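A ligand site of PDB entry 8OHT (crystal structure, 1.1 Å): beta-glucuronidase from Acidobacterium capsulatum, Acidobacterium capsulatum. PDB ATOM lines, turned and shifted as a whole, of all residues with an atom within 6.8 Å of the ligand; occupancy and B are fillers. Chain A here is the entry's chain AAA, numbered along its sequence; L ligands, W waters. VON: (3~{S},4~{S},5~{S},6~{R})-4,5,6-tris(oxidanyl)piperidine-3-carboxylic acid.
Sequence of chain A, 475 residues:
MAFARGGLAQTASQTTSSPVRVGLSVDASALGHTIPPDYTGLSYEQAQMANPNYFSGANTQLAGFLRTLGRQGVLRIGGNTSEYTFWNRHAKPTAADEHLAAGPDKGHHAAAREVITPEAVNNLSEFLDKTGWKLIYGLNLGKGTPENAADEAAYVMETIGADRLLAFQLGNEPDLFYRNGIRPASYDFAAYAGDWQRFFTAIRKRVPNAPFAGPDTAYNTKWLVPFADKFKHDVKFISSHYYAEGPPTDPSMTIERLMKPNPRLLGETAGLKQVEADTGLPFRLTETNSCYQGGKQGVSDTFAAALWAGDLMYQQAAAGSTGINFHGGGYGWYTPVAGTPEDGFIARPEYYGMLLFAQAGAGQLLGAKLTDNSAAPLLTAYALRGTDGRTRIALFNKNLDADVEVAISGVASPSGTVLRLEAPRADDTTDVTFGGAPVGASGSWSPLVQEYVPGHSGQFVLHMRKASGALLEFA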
ATOM      1  N   GLU A  45      16.990  21.876 -17.468  1.00  0.00           N
ATOM      2  CA  GLU A  45      18.088  21.064 -16.960  1.00  0.00           C
ATOM      3  C   GLU A  45      19.087  21.935 -16.243  1.00  0.00           C
ATOM      4  O   GLU A  45      19.551  22.962 -16.757  1.00  0.00           O
ATOM      5  CB  GLU A  45      18.757  20.353 -18.114  1.00  0.00           C
ATOM      6  CG  GLU A  45      17.894  19.282 -18.741  1.00  0.00           C
ATOM      7  CD  GLU A  45      17.596  18.079 -17.877  1.00  0.00           C
ATOM      8  OE1 GLU A  45      18.314  17.811 -16.911  1.00  0.00           O
ATOM      9  OE2 GLU A  45      16.616  17.379 -18.252  1.00  0.00           O
ATOM     10  N   ARG A  76      12.041  26.611 -12.772  1.00  0.00           N
ATOM     11  CA  ARG A  76      12.591  25.474 -12.019  1.00  0.00           C
ATOM     12  C   ARG A  76      13.811  24.982 -12.798  1.00  0.00           C
ATOM     13  O   ARG A  76      13.724  24.765 -14.002  1.00  0.00           O
ATOM     14  CB  ARG A  76      11.529  24.420 -11.823  1.00  0.00           C
ATOM     15  CG  ARG A  76      12.056  23.171 -11.119  1.00  0.00           C
ATOM     16  CD  ARG A  76      12.431  22.095 -12.091  1.00  0.00           C
ATOM     17  NE  ARG A  76      12.929  20.909 -11.398  1.00  0.00           N
ATOM     18  CZ  ARG A  76      13.027  19.705 -11.966  1.00  0.00           C
ATOM     19  NH1 ARG A  76      12.702  19.561 -13.201  1.00  0.00           N
ATOM     20  NH2 ARG A  76      13.497  18.692 -11.270  1.00  0.00           N
ATOM     21  N   GLY A  78      16.555  21.844 -12.659  1.00  0.00           N
ATOM     22  CA  GLY A  78      16.789  20.563 -12.029  1.00  0.00           C
ATOM     23  C   GLY A  78      16.951  19.486 -13.066  1.00  0.00           C
ATOM     24  O   GLY A  78      17.824  19.554 -13.919  1.00  0.00           O
ATOM     25  N   GLY A  79      16.097  18.474 -13.035  1.00  0.00           N
ATOM     26  CA  GLY A  79      16.140  17.423 -14.023  1.00  0.00           C
ATOM     27  C   GLY A  79      17.225  16.421 -13.767  1.00  0.00           C
ATOM     28  O   GLY A  79      17.986  16.512 -12.796  1.00  0.00           O
ATOM     29  N   ASN A  80      17.369  15.489 -14.680  1.00  0.00           N
ATOM     30  CA  ASN A  80      18.384  14.430 -14.500  1.00  0.00           C
ATOM     31  C   ASN A  80      19.770  15.007 -14.400  1.00  0.00           C
ATOM     32  O   ASN A  80      20.622  14.449 -13.728  1.00  0.00           O
ATOM     33  CB  ASN A  80      18.340  13.487 -15.705  1.00  0.00           C
ATOM     34  CG  ASN A  80      17.184  12.530 -15.678  1.00  0.00           C
ATOM     35  OD1 ASN A  80      16.449  12.506 -14.731  1.00  0.00           O
ATOM     36  ND2 ASN A  80      17.019  11.808 -16.738  1.00  0.00           N
ATOM     37  N   THR A  81      20.034  16.095 -15.119  1.00  0.00           N
ATOM     38  CA  THR A  81      21.374  16.651 -15.114  1.00  0.00           C
ATOM     39  C   THR A  81      21.713  17.228 -13.748  1.00  0.00           C
ATOM     40  O   THR A  81      22.928  17.489 -13.539  1.00  0.00           O
ATOM     41  CB  THR A  81      21.604  17.658 -16.209  1.00  0.00           C
ATOM     42  OG1 THR A  81      20.725  18.772 -16.024  1.00  0.00           O
ATOM     43  CG2 THR A  81      21.448  17.076 -17.579  1.00  0.00           C
ATOM     44  N   PRO A 104      16.560  18.946 -22.740  1.00  0.00           N
ATOM     45  CA  PRO A 104      16.091  17.890 -21.870  1.00  0.00           C
ATOM     46  C   PRO A 104      16.969  16.665 -21.925  1.00  0.00           C
ATOM     47  O   PRO A 104      17.365  16.166 -23.002  1.00  0.00           O
ATOM     48  CB  PRO A 104      14.742  17.611 -22.519  1.00  0.00           C
ATOM     49  CG  PRO A 104      14.237  18.990 -22.837  1.00  0.00           C
ATOM     50  CD  PRO A 104      15.451  19.617 -23.448  1.00  0.00           C
ATOM     51  N   ASP A 105      17.208  16.095 -20.761  1.00  0.00           N
ATOM     52  CA  ASP A 105      17.998  14.873 -20.705  1.00  0.00           C
ATOM     53  C   ASP A 105      17.167  13.742 -21.288  1.00  0.00           C
ATOM     54  O   ASP A 105      16.005  13.528 -20.918  1.00  0.00           O
ATOM     55  CB  ASP A 105      18.349  14.576 -19.275  1.00  0.00           C
ATOM     56  CG  ASP A 105      19.315  13.411 -19.178  1.00  0.00           C
ATOM     57  OD1 ASP A 105      20.527  13.635 -19.403  1.00  0.00           O
ATOM     58  OD2 ASP A 105      18.849  12.279 -18.978  1.00  0.00           O
ATOM     59  N   LYS A 106      17.764  12.970 -22.177  1.00  0.00           N
ATOM     60  CA  LYS A 106      16.998  11.934 -22.905  1.00  0.00           C
ATOM     61  C   LYS A 106      16.895  10.677 -22.054  1.00  0.00           C
ATOM     62  O   LYS A 106      16.089   9.773 -22.457  1.00  0.00           O
ATOM     63  CB  LYS A 106      17.594  11.680 -24.279  1.00  0.00           C
ATOM     64  CG  LYS A 106      17.429  12.896 -25.161  1.00  0.00           C
ATOM     65  CD  LYS A 106      18.115  12.774 -26.522  1.00  0.00           C
ATOM     66  CE  LYS A 106      17.859  13.989 -27.409  1.00  0.00           C
ATOM     67  NZ  LYS A 106      18.929  15.013 -27.330  1.00  0.00           N
ATOM     68  N   GLY A 107      17.590  10.540 -20.938  1.00  0.00           N
ATOM     69  CA  GLY A 107      17.407   9.399 -20.021  1.00  0.00           C
ATOM     70  C   GLY A 107      17.937   8.091 -20.575  1.00  0.00           C
ATOM     71  O   GLY A 107      17.448   7.051 -20.098  1.00  0.00           O
ATOM     72  N   ASN A 172      16.475  15.140  -7.982  1.00  0.00           N
ATOM     73  CA  ASN A 172      15.415  15.047  -8.979  1.00  0.00           C
ATOM     74  C   ASN A 172      15.038  13.602  -9.115  1.00  0.00           C
ATOM     75  O   ASN A 172      15.907  12.750  -9.285  1.00  0.00           O
ATOM     76  CB  ASN A 172      15.967  15.586 -10.285  1.00  0.00           C
ATOM     77  CG  ASN A 172      15.063  15.278 -11.451  1.00  0.00           C
ATOM     78  OD1 ASN A 172      14.051  15.978 -11.670  1.00  0.00           O
ATOM     79  ND2 ASN A 172      15.428  14.292 -12.228  1.00  0.00           N
ATOM     80  N   GLU A 173      13.756  13.287  -9.088  1.00  0.00           N
ATOM     81  CA  GLU A 173      13.266  11.926  -9.337  1.00  0.00           C
ATOM     82  C   GLU A 173      14.125  10.904  -8.603  1.00  0.00           C
ATOM     83  O   GLU A 173      14.630   9.957  -9.173  1.00  0.00           O
ATOM     84  CB  GLU A 173      13.201  11.658 -10.819  1.00  0.00           C
ATOM     85  CG  GLU A 173      12.223  12.584 -11.501  1.00  0.00           C
ATOM     86  CD  GLU A 173      11.943  12.390 -12.968  1.00  0.00           C
ATOM     87  OE1 GLU A 173      12.703  11.733 -13.660  1.00  0.00           O
ATOM     88  OE2 GLU A 173      10.974  13.018 -13.466  1.00  0.00           O
ATOM     89  N   LEU A 176      13.996   7.141  -9.161  1.00  0.00           N
ATOM     90  CA  LEU A 176      14.584   6.595 -10.374  1.00  0.00           C
ATOM     91  C   LEU A 176      16.089   6.615 -10.288  1.00  0.00           C
ATOM     92  O   LEU A 176      16.760   6.338 -11.365  1.00  0.00           O
ATOM     93  CB  LEU A 176      14.143   7.346 -11.592  1.00  0.00           C
ATOM     94  CG  LEU A 176      12.629   7.412 -11.743  1.00  0.00           C
ATOM     95  CD1 LEU A 176      12.283   8.202 -12.988  1.00  0.00           C
ATOM     96  CD2 LEU A 176      12.009   6.028 -11.810  1.00  0.00           C
ATOM     97  N   ASP A 216      10.033  15.903  -5.693  1.00  0.00           N
ATOM     98  CA  ASP A 216      10.472  16.158  -7.070  1.00  0.00           C
ATOM     99  C   ASP A 216      10.386  14.892  -7.888  1.00  0.00           C
ATOM    100  O   ASP A 216      11.275  14.623  -8.742  1.00  0.00           O
ATOM    101  CB  ASP A 216      11.873  16.760  -7.128  1.00  0.00           C
ATOM    102  CG  ASP A 216      12.084  17.711  -8.301  1.00  0.00           C
ATOM    103  OD1 ASP A 216      11.093  18.281  -8.858  1.00  0.00           O
ATOM    104  OD2 ASP A 216      13.292  17.868  -8.636  1.00  0.00           O
ATOM    105  N   HIS A 241       6.008  15.448 -10.486  1.00  0.00           N
ATOM    106  CA  HIS A 241       6.243  15.467 -11.928  1.00  0.00           C
ATOM    107  C   HIS A 241       5.120  14.722 -12.626  1.00  0.00           C
ATOM    108  O   HIS A 241       4.441  13.874 -12.022  1.00  0.00           O
ATOM    109  CB  HIS A 241       7.540  14.764 -12.307  1.00  0.00           C
ATOM    110  CG  HIS A 241       8.738  15.485 -11.769  1.00  0.00           C
ATOM    111  ND1 HIS A 241      10.032  15.101 -12.108  1.00  0.00           N
ATOM    112  CD2 HIS A 241       8.880  16.576 -10.992  1.00  0.00           C
ATOM    113  CE1 HIS A 241      10.872  15.939 -11.537  1.00  0.00           C
ATOM    114  NE2 HIS A 241      10.229  16.829 -10.867  1.00  0.00           N
ATOM    115  N   TYR A 243       4.296  13.130 -16.724  1.00  0.00           N
ATOM    116  CA  TYR A 243       4.380  12.994 -18.183  1.00  0.00           C
ATOM    117  C   TYR A 243       3.151  12.237 -18.652  1.00  0.00           C
ATOM    118  O   TYR A 243       2.747  11.231 -17.999  1.00  0.00           O
ATOM    119  CB  TYR A 243       5.664  12.300 -18.604  1.00  0.00           C
ATOM    120  CG  TYR A 243       6.844  13.204 -18.525  1.00  0.00           C
ATOM    121  CD1 TYR A 243       7.410  13.527 -17.326  1.00  0.00           C
ATOM    122  CD2 TYR A 243       7.316  13.851 -19.633  1.00  0.00           C
ATOM    123  CE1 TYR A 243       8.409  14.485 -17.191  1.00  0.00           C
ATOM    124  CE2 TYR A 243       8.291  14.807 -19.533  1.00  0.00           C
ATOM    125  CZ  TYR A 243       8.823  15.125 -18.319  1.00  0.00           C
ATOM    126  OH  TYR A 243       9.774  16.109 -18.258  1.00  0.00           O
ATOM    127  N   GLU A 287       7.753  19.534 -12.815  1.00  0.00           N
ATOM    128  CA  GLU A 287       8.342  19.103 -14.085  1.00  0.00           C
ATOM    129  C   GLU A 287       7.264  18.345 -14.810  1.00  0.00           C
ATOM    130  O   GLU A 287       6.817  17.296 -14.339  1.00  0.00           O
ATOM    131  CB  GLU A 287       9.583  18.266 -13.912  1.00  0.00           C
ATOM    132  CG  GLU A 287      10.322  18.126 -15.228  1.00  0.00           C
ATOM    133  CD  GLU A 287      11.331  17.009 -15.206  1.00  0.00           C
ATOM    134  OE1 GLU A 287      12.334  17.072 -14.495  1.00  0.00           O
ATOM    135  OE2 GLU A 287      11.078  16.036 -15.974  1.00  0.00           O
ATOM    136  N   ASN A 289       5.868  17.249 -19.042  1.00  0.00           N
ATOM    137  CA  ASN A 289       5.665  17.465 -20.457  1.00  0.00           C
ATOM    138  C   ASN A 289       4.944  16.272 -21.027  1.00  0.00           C
ATOM    139  O   ASN A 289       4.519  15.373 -20.301  1.00  0.00           O
ATOM    140  CB  ASN A 289       6.946  17.905 -21.183  1.00  0.00           C
ATOM    141  CG  ASN A 289       6.615  19.034 -22.110  1.00  0.00           C
ATOM    142  OD1 ASN A 289       5.625  18.905 -22.845  1.00  0.00           O
ATOM    143  ND2 ASN A 289       7.349  20.122 -22.081  1.00  0.00           N
ATOM    144  N   CYS A 291       5.753  13.740 -23.379  1.00  0.00           N
ATOM    145  CA  CYS A 291       6.398  12.440 -23.633  1.00  0.00           C
ATOM    146  C   CYS A 291       7.781  12.473 -23.023  1.00  0.00           C
ATOM    147  O   CYS A 291       8.438  13.484 -23.024  1.00  0.00           O
ATOM    148  CB  CYS A 291       6.497  12.160 -25.132  1.00  0.00           C
ATOM    149  SG  CYS A 291       4.907  12.141 -25.968  1.00  0.00           S
ATOM    150  N   TYR A 292       8.257  11.320 -22.576  1.00  0.00           N
ATOM    151  CA  TYR A 292       9.606  11.159 -22.016  1.00  0.00           C
ATOM    152  C   TYR A 292      10.708  11.261 -23.043  1.00  0.00           C
ATOM    153  O   TYR A 292      10.534  11.353 -24.263  1.00  0.00           O
ATOM    154  CB  TYR A 292       9.771   9.777 -21.399  1.00  0.00           C
ATOM    155  CG  TYR A 292       8.942   9.669 -20.175  1.00  0.00           C
ATOM    156  CD1 TYR A 292       9.338  10.370 -19.041  1.00  0.00           C
ATOM    157  CD2 TYR A 292       7.854   8.842 -20.128  1.00  0.00           C
ATOM    158  CE1 TYR A 292       8.656  10.233 -17.852  1.00  0.00           C
ATOM    159  CE2 TYR A 292       7.144   8.716 -18.951  1.00  0.00           C
ATOM    160  CZ  TYR A 292       7.533   9.442 -17.834  1.00  0.00           C
ATOM    161  OH  TYR A 292       6.934   9.317 -16.598  1.00  0.00           O
ATOM    162  N   GLN A 293      11.930  11.266 -22.507  1.00  0.00           N
ATOM    163  CA  GLN A 293      13.176  11.226 -23.294  1.00  0.00           C
ATOM    164  C   GLN A 293      13.358  12.472 -24.135  1.00  0.00           C
ATOM    165  O   GLN A 293      13.851  12.402 -25.287  1.00  0.00           O
ATOM    166  CB  GLN A 293      13.317   9.929 -24.083  1.00  0.00           C
ATOM    167  CG  GLN A 293      12.913   8.729 -23.246  1.00  0.00           C
ATOM    168  CD  GLN A 293      13.141   7.404 -23.944  1.00  0.00           C
ATOM    169  OE1 GLN A 293      13.485   7.345 -25.117  1.00  0.00           O
ATOM    170  NE2 GLN A 293      12.919   6.318 -23.229  1.00  0.00           N
ATOM    171  N   GLY A 294      12.902  13.608 -23.671  1.00  0.00           N
ATOM    172  CA  GLY A 294      13.006  14.868 -24.397  1.00  0.00           C
ATOM    173  C   GLY A 294      11.819  15.037 -25.345  1.00  0.00           C
ATOM    174  O   GLY A 294      11.721  16.143 -25.951  1.00  0.00           O
ATOM    175  N   GLY A 295      10.882  14.070 -25.296  1.00  0.00           N
ATOM    176  CA  GLY A 295       9.697  14.165 -26.136  1.00  0.00           C
ATOM    177  C   GLY A 295       9.700  13.236 -27.309  1.00  0.00           C
ATOM    178  O   GLY A 295      10.761  12.695 -27.658  1.00  0.00           O
ATOM    179  N   HIS A 327       8.828  21.189 -18.776  1.00  0.00           N
ATOM    180  CA  HIS A 327      10.259  20.930 -19.013  1.00  0.00           C
ATOM    181  C   HIS A 327      10.625  21.255 -20.438  1.00  0.00           C
ATOM    182  O   HIS A 327       9.826  21.161 -21.352  1.00  0.00           O
ATOM    183  CB  HIS A 327      10.618  19.528 -18.609  1.00  0.00           C
ATOM    184  CG  HIS A 327      12.047  19.313 -18.307  1.00  0.00           C
ATOM    185  ND1 HIS A 327      12.679  20.042 -17.317  1.00  0.00           N
ATOM    186  CD2 HIS A 327      12.936  18.476 -18.864  1.00  0.00           C
ATOM    187  CE1 HIS A 327      13.928  19.600 -17.303  1.00  0.00           C
ATOM    188  NE2 HIS A 327      14.113  18.670 -18.220  1.00  0.00           N
ATOM    189  N   TYR A 334       9.864  18.491 -26.824  1.00  0.00           N
ATOM    190  CA  TYR A 334       8.739  19.043 -26.068  1.00  0.00           C
ATOM    191  C   TYR A 334       8.977  20.464 -25.564  1.00  0.00           C
ATOM    192  O   TYR A 334       8.139  20.978 -24.834  1.00  0.00           O
ATOM    193  CB  TYR A 334       8.281  18.135 -24.934  1.00  0.00           C
ATOM    194  CG  TYR A 334       9.281  17.727 -23.904  1.00  0.00           C
ATOM    195  CD1 TYR A 334      10.107  18.616 -23.241  1.00  0.00           C
ATOM    196  CD2 TYR A 334       9.365  16.390 -23.549  1.00  0.00           C
ATOM    197  CE1 TYR A 334      11.007  18.171 -22.287  1.00  0.00           C
ATOM    198  CE2 TYR A 334      10.235  15.924 -22.594  1.00  0.00           C
ATOM    199  CZ  TYR A 334      11.078  16.843 -21.974  1.00  0.00           C
ATOM    200  OH  TYR A 334      11.967  16.447 -21.010  1.00  0.00           O
HETATM  201  O11 VON L   1      12.180  11.968 -19.778  1.00  0.00           O
HETATM  202  N1  VON L   1      12.447  13.733 -16.060  1.00  0.00           N
HETATM  203  C2  VON L   1      13.829  14.188 -15.874  1.00  0.00           C
HETATM  204  C3  VON L   1      14.240  15.051 -17.036  1.00  0.00           C
HETATM  205  C4  VON L   1      13.966  14.377 -18.372  1.00  0.00           C
HETATM  206  C5  VON L   1      12.509  13.939 -18.462  1.00  0.00           C
HETATM  207  C6  VON L   1      12.264  13.224 -19.792  1.00  0.00           C
HETATM  208  C7  VON L   1      12.157  13.026 -17.292  1.00  0.00           C
HETATM  209  O8  VON L   1      13.907  14.831 -14.649  1.00  0.00           O
HETATM  210  O9  VON L   1      15.600  15.331 -16.851  1.00  0.00           O
HETATM  211  O10 VON L   1      14.807  13.239 -18.506  1.00  0.00           O
HETATM  212  O12 VON L   1      12.229  13.893 -20.829  1.00  0.00           O
HETATM  213  O   HOH W   1      11.821   9.979 -15.834  1.00  0.00           O
HETATM  214  O   HOH W   2      12.555   9.750 -18.415  1.00  0.00           O
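O of Tyr 334 lies within hydrogen-bond range of ND2 of Asn 289 (3.0 Å). A ring nitrogen (NE2) of His 327 lies within hydrogen-bond range of the side-chain carboxylate (OE2) of Glu 45, at 2.8 Å. N of Asp 105 sits at hydrogen-bond distance from OE2 of Glu 45 (2.9 Å). A ring nitrogen (ND1) of His 241 sits at hydrogen-bond distance from the side-chain carboxylate (OE2) of Glu 173, at 2.7 Å. The backbone NH (N) of Glu 173 lies within hydrogen-bond range of the backbone carbonyl oxygen (O) of Asp 216, at 2.8 Å. The backbone carbonyl oxygen (O) of Gly 294 lies within hydrogen-bond range of the backbone NH (N) of Tyr 334 (3.1 Å). The side-chain amide oxygen (OD1) of Asn 172 sits close to the side-chain carboxylate (OE1) of Glu 287, at 3.5 Å. The backbone carbonyl oxygen of His 327 lies within hydrogen-bond range of the side-chain amide nitrogen of Asn 289 (2.8 Å).
The backbone NH (N) of Gln 293 sits at hydrogen-bond distance from an oxygen (O11) of the ligand, at 2.8 Å. The side-chain hydroxyl (OH) of Tyr 334 sits at hydrogen-bond distance from an oxygen (O12) of the ligand (2.6 Å). A nitrogen (N1) of the ligand is in salt-bridge range of the side-chain carboxylate of Glu 173. ND2 of Asn 172 is in hydrogen-bond range of O8 of the ligand, at 2.9 Å. The backbone carbonyl oxygen (O) of Asp 105 lies within hydrogen-bond range of an oxygen (O10) of the ligand, 2.7 Å away. The side-chain carboxylate of Glu 287 lies within salt-bridge range of a nitrogen (N1) of the ligand, 2.7 Å away. The side-chain amide nitrogen (ND2) of Asn 80 lies within hydrogen-bond range of an oxygen (O10) of the ligand (3.2 Å). O9 of the ligand sits at hydrogen-bond distance from OE2 of Glu 45 (2.7 Å). O9 of the ligand lies within hydrogen-bond range of N of Asn 80 (2.8 Å). The backbone NH (N) of Gly 294 is in hydrogen-bond range of an oxygen (O12) of the ligand (2.9 Å).
Gly 79 touches the ligand (CA to O8, 3.5 Å). Tyr 243 touches the ligand (OH to C5, 3.5 Å). Tyr 292 touches the ligand (CD1 to O11, 3.3 Å). His 327 touches the ligand (NE2 to C3, 3.8 Å). Hydrophobic or aromatic side chains that line the ligand: Tyr 243, Tyr 292 and Tyr 334. Of the 25 residues printed, 13 come within 4 Å of the ligand.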
